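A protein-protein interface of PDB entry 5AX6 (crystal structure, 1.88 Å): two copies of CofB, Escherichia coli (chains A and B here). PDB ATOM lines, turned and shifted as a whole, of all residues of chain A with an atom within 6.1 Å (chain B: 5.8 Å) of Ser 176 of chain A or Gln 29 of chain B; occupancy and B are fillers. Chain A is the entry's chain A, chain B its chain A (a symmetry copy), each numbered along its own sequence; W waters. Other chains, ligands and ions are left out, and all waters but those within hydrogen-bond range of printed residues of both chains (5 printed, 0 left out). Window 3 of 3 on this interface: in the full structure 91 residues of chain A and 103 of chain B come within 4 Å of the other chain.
Of chain B, only Gln 29 (3.6 Å) comes within 4 Å of Ser 176 of chain A. Of chain A, only Ser 176, Leu 231 and Arg 240 come within 4 Å of Gln 29 of chain B. Of the printed residues of chain B, Leu 231 of chain A touches Glu 28 (3.98 Å) and Gln 29 (3.96 Å). Of the printed residues of chain A, Ile 30 of chain B touches Arg 240 (3.5 Å). Printed residues of chain B within 4 Å of Arg 240 of chain A: Glu 27 (3.5 Å), Gln 29 (2.9 Å), Ile 30 (3.5 Å), Thr 31 (2.9 Å) and Glu 40 (2.9 Å). The nearest residue of chain B that does not touch Ser 176 of chain A is Thr 42 of chain B (5.5 Å). The nearest residue of chain A that does not touch Gln 29 of chain B is Phe 177 of chain A (5.7 Å). The nearest printed residue of chain A that does not touch Ile 30 of chain B is Leu 231 of chain A (8.3 Å).
The side-chain carboxylate of Glu 27 of chain B lies within salt-bridge range of the guanidinium group of Arg 240 of chain A. The backbone carbonyl oxygen (O) of Gln 29 of chain B lies within hydrogen-bond range of the guanidinium group (NH2) of Arg 240 of chain A (2.9 Å). OG1 of Thr 31 of chain B lies within hydrogen-bond range of NH1 of Arg 240 of chain A (2.9 Å). The guanidinium group of Arg 240 of chain A is in salt-bridge range of the side-chain carboxylate of Glu 40 of chain B, at 2.9 Å.
No position is printed for both chains. Of the 8 pairs that touch across the chains among the printed residues, none has its exchanged pair printed and touching as well.
Among the printed residues, merely in contact across the chains: Arg 240 of chain A with Ile 30 of chain B (3.5 Å), Ser 176 of chain A with Gln 29 of chain B (3.6 Å), Leu 231 of chain A with Gln 29 of chain B (3.96 Å) and Leu 231 of chain A with Glu 28 of chain B (3.98 Å).
The side-chain amide nitrogen (ND2) of Asn 43 of chain B is in hydrogen-bond range of the backbone carbonyl oxygen (O) of Glu 27 of chain B. The backbone carbonyl oxygen (O) of Glu 28 of chain B is in hydrogen-bond range of the backbone NH (N) of Asn 43 of chain B, 2.7 Å away. The side-chain amide oxygen (OE1) of Gln 29 of chain B is in hydrogen-bond range of the side-chain hydroxyl (OG1) of Thr 42 of chain B, at 3.1 Å. The backbone NH (N) of Ile 30 of chain B sits at hydrogen-bond distance from the backbone carbonyl oxygen (O) of Ile 41 of chain B, at 2.8 Å. OG1 of Thr 31 of chain B is in hydrogen-bond range of OE2 of Glu 40 of chain B (2.7 Å).
Water W4 bridges OE2 of Glu 28 of chain B (2.4 Å) and OD2 of Asp 228 of chain A (2.9 Å). Water W1 lies within hydrogen-bond range of the side-chain hydroxyl (OG1) of Thr 42 of chain B (2.4 Å), the backbone carbonyl oxygen (O) of Phe 177 of chain A (2.7 Å) and the backbone carbonyl oxygen (O) of Lys 178 of chain A (3.3 Å). Water W5 lies within hydrogen-bond range of NE of Arg 240 of chain A (2.7 Å) and O of Gln 29 of chain B (2.8 Å). Water W3 lies within hydrogen-bond range of the side-chain carboxylate (OE2) of Glu 28 of chain B (2.8 Å) and the side-chain amino group (NZ) of Lys 178 of chain A (3.4 Å). Water W2 lies within hydrogen-bond range of the side-chain carboxylate (OE1) of Glu 27 of chain B (2.8 Å), the backbone NH (N) of Thr 31 of chain B (2.8 Å) and the guanidinium group (NH1) of Arg 240 of chain A (3.2 Å).
Printed residues of chain A that touch a printed residue of chain B: Ser 176, Leu 231 and Arg 240. Hydrophobic or aromatic side chains of chain A within 4 Å of the printed part of chain B: Leu 231. Among the printed residues, 8 pairs touch across the chains.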
ATOM      1  N   ALA A 170       0.011  14.579 -24.158  1.00  0.00           N
ATOM      2  CA  ALA A 170       1.062  14.941 -23.221  1.00  0.00           C
ATOM      3  C   ALA A 170       0.482  15.198 -21.833  1.00  0.00           C
ATOM      4  O   ALA A 170       1.052  14.778 -20.829  1.00  0.00           O
ATOM      5  CB  ALA A 170       1.835  16.158 -23.721  1.00  0.00           C
ATOM      6  N   SER A 174       1.646  13.331 -17.888  1.00  0.00           N
ATOM      7  CA  SER A 174       2.483  14.096 -16.960  1.00  0.00           C
ATOM      8  C   SER A 174       3.739  14.636 -17.610  1.00  0.00           C
ATOM      9  O   SER A 174       4.793  14.687 -16.982  1.00  0.00           O
ATOM     10  CB  SER A 174       2.879  13.240 -15.752  1.00  0.00           C
ATOM     11  OG  SER A 174       1.741  12.908 -14.982  1.00  0.00           O
ATOM     12  N   ILE A 175       3.642  15.015 -18.875  1.00  0.00           N
ATOM     13  CA  ILE A 175       4.766  15.678 -19.515  1.00  0.00           C
ATOM     14  C   ILE A 175       4.258  16.868 -20.286  1.00  0.00           C
ATOM     15  O   ILE A 175       3.065  16.987 -20.551  1.00  0.00           O
ATOM     16  CB  ILE A 175       5.537  14.752 -20.463  1.00  0.00           C
ATOM     17  CG1 ILE A 175       4.641  14.307 -21.620  1.00  0.00           C
ATOM     18  CG2 ILE A 175       6.104  13.564 -19.709  1.00  0.00           C
ATOM     19  CD1 ILE A 175       5.445  13.822 -22.818  1.00  0.00           C
ATOM     20  N   SER A 176       5.172  17.751 -20.655  1.00  0.00           N
ATOM     21  CA  SER A 176       4.791  18.938 -21.386  1.00  0.00           C
ATOM     22  C   SER A 176       5.916  19.316 -22.327  1.00  0.00           C
ATOM     23  O   SER A 176       7.053  18.870 -22.173  1.00  0.00           O
ATOM     24  CB  SER A 176       4.469  20.090 -20.428  1.00  0.00           C
ATOM     25  OG  SER A 176       5.604  20.427 -19.656  1.00  0.00           O
ATOM     26  N   PHE A 177       5.595  20.126 -23.320  1.00  0.00           N
ATOM     27  CA  PHE A 177       6.617  20.536 -24.275  1.00  0.00           C
ATOM     28  C   PHE A 177       7.223  21.870 -23.888  1.00  0.00           C
ATOM     29  O   PHE A 177       6.500  22.838 -23.661  1.00  0.00           O
ATOM     30  CB  PHE A 177       6.027  20.616 -25.671  1.00  0.00           C
ATOM     31  CG  PHE A 177       5.321  19.359 -26.094  1.00  0.00           C
ATOM     32  CD1 PHE A 177       6.026  18.171 -26.231  1.00  0.00           C
ATOM     33  CD2 PHE A 177       3.963  19.370 -26.372  1.00  0.00           C
ATOM     34  CE1 PHE A 177       5.382  17.009 -26.626  1.00  0.00           C
ATOM     35  CE2 PHE A 177       3.312  18.215 -26.766  1.00  0.00           C
ATOM     36  CZ  PHE A 177       4.016  17.032 -26.889  1.00  0.00           C
ATOM     37  N   LYS A 178       8.552  21.914 -23.821  1.00  0.00           N
ATOM     38  CA  LYS A 178       9.266  23.159 -23.575  1.00  0.00           C
ATOM     39  C   LYS A 178       8.946  24.132 -24.706  1.00  0.00           C
ATOM     40  O   LYS A 178       8.672  25.313 -24.480  1.00  0.00           O
ATOM     41  CB  LYS A 178      10.770  22.906 -23.470  1.00  0.00           C
ATOM     42  CG  LYS A 178      11.578  24.137 -23.072  1.00  0.00           C
ATOM     43  CD  LYS A 178      13.073  23.859 -23.145  1.00  0.00           C
ATOM     44  CE  LYS A 178      13.880  25.083 -22.746  1.00  0.00           C
ATOM     45  NZ  LYS A 178      13.878  25.237 -21.271  1.00  0.00           N
ATOM     46  N   SER A 226      10.287  19.609 -28.051  1.00  0.00           N
ATOM     47  CA  SER A 226      11.362  19.648 -27.057  1.00  0.00           C
ATOM     48  C   SER A 226      10.836  19.303 -25.675  1.00  0.00           C
ATOM     49  O   SER A 226       9.849  19.884 -25.231  1.00  0.00           O
ATOM     50  CB  SER A 226      12.019  21.034 -27.004  1.00  0.00           C
ATOM     51  OG  SER A 226      12.594  21.374 -28.252  1.00  0.00           O
ATOM     52  N   ILE A 227      11.505  18.371 -25.004  1.00  0.00           N
ATOM     53  CA  ILE A 227      11.141  17.993 -23.636  1.00  0.00           C
ATOM     54  C   ILE A 227      12.293  18.265 -22.683  1.00  0.00           C
ATOM     55  O   ILE A 227      13.441  17.920 -22.972  1.00  0.00           O
ATOM     56  CB  ILE A 227      10.778  16.503 -23.515  1.00  0.00           C
ATOM     57  CG1 ILE A 227       9.858  16.062 -24.656  1.00  0.00           C
ATOM     58  CG2 ILE A 227      10.207  16.215 -22.118  1.00  0.00           C
ATOM     59  CD1 ILE A 227       8.415  16.502 -24.508  1.00  0.00           C
ATOM     60  N   ASP A 228      11.989  18.882 -21.546  1.00  0.00           N
ATOM     61  CA  ASP A 228      12.969  19.061 -20.475  1.00  0.00           C
ATOM     62  C   ASP A 228      12.929  17.825 -19.583  1.00  0.00           C
ATOM     63  O   ASP A 228      11.964  17.645 -18.852  1.00  0.00           O
ATOM     64  CB  ASP A 228      12.638  20.330 -19.662  1.00  0.00           C
ATOM     65  CG  ASP A 228      13.615  20.591 -18.525  1.00  0.00           C
ATOM     66  OD1 ASP A 228      14.502  19.746 -18.253  1.00  0.00           O
ATOM     67  OD2 ASP A 228      13.478  21.658 -17.882  1.00  0.00           O
ATOM     68  N   LEU A 231      12.108  18.435 -15.830  1.00  0.00           N
ATOM     69  CA  LEU A 231      10.856  19.039 -15.403  1.00  0.00           C
ATOM     70  C   LEU A 231       9.938  17.966 -14.817  1.00  0.00           C
ATOM     71  O   LEU A 231       9.610  16.995 -15.496  1.00  0.00           O
ATOM     72  CB  LEU A 231      10.174  19.752 -16.573  1.00  0.00           C
ATOM     73  CG  LEU A 231       8.868  20.490 -16.246  1.00  0.00           C
ATOM     74  CD1 LEU A 231       9.111  21.591 -15.208  1.00  0.00           C
ATOM     75  CD2 LEU A 231       8.267  21.073 -17.519  1.00  0.00           C
ATOM     76  N   ARG A 240       3.350  19.665  -6.015  1.00  0.00           N
ATOM     77  CA  ARG A 240       2.787  19.699  -7.370  1.00  0.00           C
ATOM     78  C   ARG A 240       3.275  18.579  -8.312  1.00  0.00           C
ATOM     79  O   ARG A 240       2.855  18.517  -9.464  1.00  0.00           O
ATOM     80  CB  ARG A 240       3.052  21.077  -8.001  1.00  0.00           C
ATOM     81  CG  ARG A 240       2.223  22.196  -7.335  1.00  0.00           C
ATOM     82  CD  ARG A 240       2.517  23.588  -7.913  1.00  0.00           C
ATOM     83  NE  ARG A 240       2.390  23.623  -9.368  1.00  0.00           N
ATOM     84  CZ  ARG A 240       1.230  23.567 -10.017  1.00  0.00           C
ATOM     85  NH1 ARG A 240       0.092  23.471  -9.338  1.00  0.00           N
ATOM     86  NH2 ARG A 240       1.207  23.596 -11.342  1.00  0.00           N
ATOM     87  N   GLU B  27       7.656  27.820 -10.125  1.00  0.00           N
ATOM     88  CA  GLU B  27       6.724  26.936 -10.828  1.00  0.00           C
ATOM     89  C   GLU B  27       6.803  27.157 -12.330  1.00  0.00           C
ATOM     90  O   GLU B  27       6.255  28.125 -12.844  1.00  0.00           O
ATOM     91  CB  GLU B  27       5.281  27.147 -10.335  1.00  0.00           C
ATOM     92  CG  GLU B  27       5.083  26.757  -8.888  1.00  0.00           C
ATOM     93  CD  GLU B  27       3.674  27.040  -8.359  1.00  0.00           C
ATOM     94  OE1 GLU B  27       2.778  27.389  -9.160  1.00  0.00           O
ATOM     95  OE2 GLU B  27       3.474  26.910  -7.133  1.00  0.00           O
ATOM     96  N   GLU B  28       7.482  26.264 -13.046  1.00  0.00           N
ATOM     97  CA  GLU B  28       7.538  26.401 -14.492  1.00  0.00           C
ATOM     98  C   GLU B  28       6.204  26.043 -15.130  1.00  0.00           C
ATOM     99  O   GLU B  28       5.811  26.634 -16.139  1.00  0.00           O
ATOM    100  CB  GLU B  28       8.648  25.538 -15.084  1.00  0.00           C
ATOM    101  CG  GLU B  28       8.703  25.627 -16.590  1.00  0.00           C
ATOM    102  CD  GLU B  28      10.101  25.401 -17.131  1.00  0.00           C
ATOM    103  OE1 GLU B  28      11.039  25.264 -16.316  1.00  0.00           O
ATOM    104  OE2 GLU B  28      10.257  25.365 -18.369  1.00  0.00           O
ATOM    105  N   GLN B  29       5.522  25.064 -14.543  1.00  0.00           N
ATOM    106  CA  GLN B  29       4.160  24.722 -14.923  1.00  0.00           C
ATOM    107  C   GLN B  29       3.222  25.230 -13.835  1.00  0.00           C
ATOM    108  O   GLN B  29       3.450  24.972 -12.653  1.00  0.00           O
ATOM    109  CB  GLN B  29       4.003  23.209 -15.107  1.00  0.00           C
ATOM    110  CG  GLN B  29       4.860  22.623 -16.232  1.00  0.00           C
ATOM    111  CD  GLN B  29       4.460  23.127 -17.617  1.00  0.00           C
ATOM    112  OE1 GLN B  29       5.186  23.905 -18.249  1.00  0.00           O
ATOM    113  NE2 GLN B  29       3.313  22.676 -18.099  1.00  0.00           N
ATOM    114  N   ILE B  30       2.182  25.964 -14.216  1.00  0.00           N
ATOM    115  CA  ILE B  30       1.272  26.517 -13.212  1.00  0.00           C
ATOM    116  C   ILE B  30      -0.165  26.125 -13.482  1.00  0.00           C
ATOM    117  O   ILE B  30      -0.526  25.823 -14.617  1.00  0.00           O
ATOM    118  CB  ILE B  30       1.346  28.066 -13.145  1.00  0.00           C
ATOM    119  CG1 ILE B  30       1.036  28.674 -14.510  1.00  0.00           C
ATOM    120  CG2 ILE B  30       2.716  28.501 -12.697  1.00  0.00           C
ATOM    121  CD1 ILE B  30       0.936  30.194 -14.484  1.00  0.00           C
ATOM    122  N   THR B  31      -0.981  26.148 -12.431  1.00  0.00           N
ATOM    123  CA  THR B  31      -2.405  25.870 -12.559  1.00  0.00           C
ATOM    124  C   THR B  31      -3.181  27.183 -12.690  1.00  0.00           C
ATOM    125  O   THR B  31      -3.090  28.052 -11.827  1.00  0.00           O
ATOM    126  CB  THR B  31      -2.949  25.071 -11.345  1.00  0.00           C
ATOM    127  OG1 THR B  31      -2.184  23.872 -11.168  1.00  0.00           O
ATOM    128  CG2 THR B  31      -4.411  24.698 -11.568  1.00  0.00           C
ATOM    129  N   GLU B  40      -3.320  23.123 -16.613  1.00  0.00           N
ATOM    130  CA  GLU B  40      -1.890  23.363 -16.457  1.00  0.00           C
ATOM    131  C   GLU B  40      -1.368  24.082 -17.678  1.00  0.00           C
ATOM    132  O   GLU B  40      -1.609  23.657 -18.810  1.00  0.00           O
ATOM    133  CB  GLU B  40      -1.106  22.059 -16.265  1.00  0.00           C
ATOM    134  CG  GLU B  40      -1.587  21.197 -15.129  1.00  0.00           C
ATOM    135  CD  GLU B  40      -1.466  21.887 -13.795  1.00  0.00           C
ATOM    136  OE1 GLU B  40      -0.321  22.133 -13.352  1.00  0.00           O
ATOM    137  OE2 GLU B  40      -2.521  22.184 -13.188  1.00  0.00           O
ATOM    138  N   ILE B  41      -0.643  25.174 -17.452  1.00  0.00           N
ATOM    139  CA  ILE B  41       0.040  25.845 -18.540  1.00  0.00           C
ATOM    140  C   ILE B  41       1.478  26.158 -18.153  1.00  0.00           C
ATOM    141  O   ILE B  41       1.855  26.111 -16.980  1.00  0.00           O
ATOM    142  CB  ILE B  41      -0.660  27.165 -18.941  1.00  0.00           C
ATOM    143  CG1 ILE B  41      -0.658  28.137 -17.749  1.00  0.00           C
ATOM    144  CG2 ILE B  41      -2.071  26.893 -19.444  1.00  0.00           C
ATOM    145  CD1 ILE B  41      -1.033  29.557 -18.127  1.00  0.00           C
ATOM    146  N   THR B  42       2.283  26.456 -19.157  1.00  0.00           N
ATOM    147  CA  THR B  42       3.609  26.968 -18.905  1.00  0.00           C
ATOM    148  C   THR B  42       3.487  28.350 -18.251  1.00  0.00           C
ATOM    149  O   THR B  42       2.735  29.201 -18.724  1.00  0.00           O
ATOM    150  CB  THR B  42       4.411  27.051 -20.203  1.00  0.00           C
ATOM    151  OG1 THR B  42       4.616  25.723 -20.705  1.00  0.00           O
ATOM    152  CG2 THR B  42       5.758  27.724 -19.964  1.00  0.00           C
ATOM    153  N   ASN B  43       4.220  28.555 -17.163  1.00  0.00           N
ATOM    154  CA  ASN B  43       4.343  29.882 -16.548  1.00  0.00           C
ATOM    155  C   ASN B  43       4.737  30.920 -17.613  1.00  0.00           C
ATOM    156  O   ASN B  43       5.684  30.702 -18.372  1.00  0.00           O
ATOM    157  CB  ASN B  43       5.380  29.830 -15.414  1.00  0.00           C
ATOM    158  CG  ASN B  43       5.362  31.070 -14.532  1.00  0.00           C
ATOM    159  OD1 ASN B  43       5.176  32.190 -15.011  1.00  0.00           O
ATOM    160  ND2 ASN B  43       5.572  30.869 -13.230  1.00  0.00           N
HETATM  161  O   HOH W   1       5.895  25.279 -22.742  1.00  0.00           O
HETATM  162  O   HOH W   2       0.151  26.674  -9.884  1.00  0.00           O
HETATM  163  O   HOH W   3      11.044  26.922 -20.511  1.00  0.00           O
HETATM  164  O   HOH W   4      11.589  23.476 -19.061  1.00  0.00           O
HETATM  165  O   HOH W   5       4.720  23.324 -10.770  1.00  0.00           O
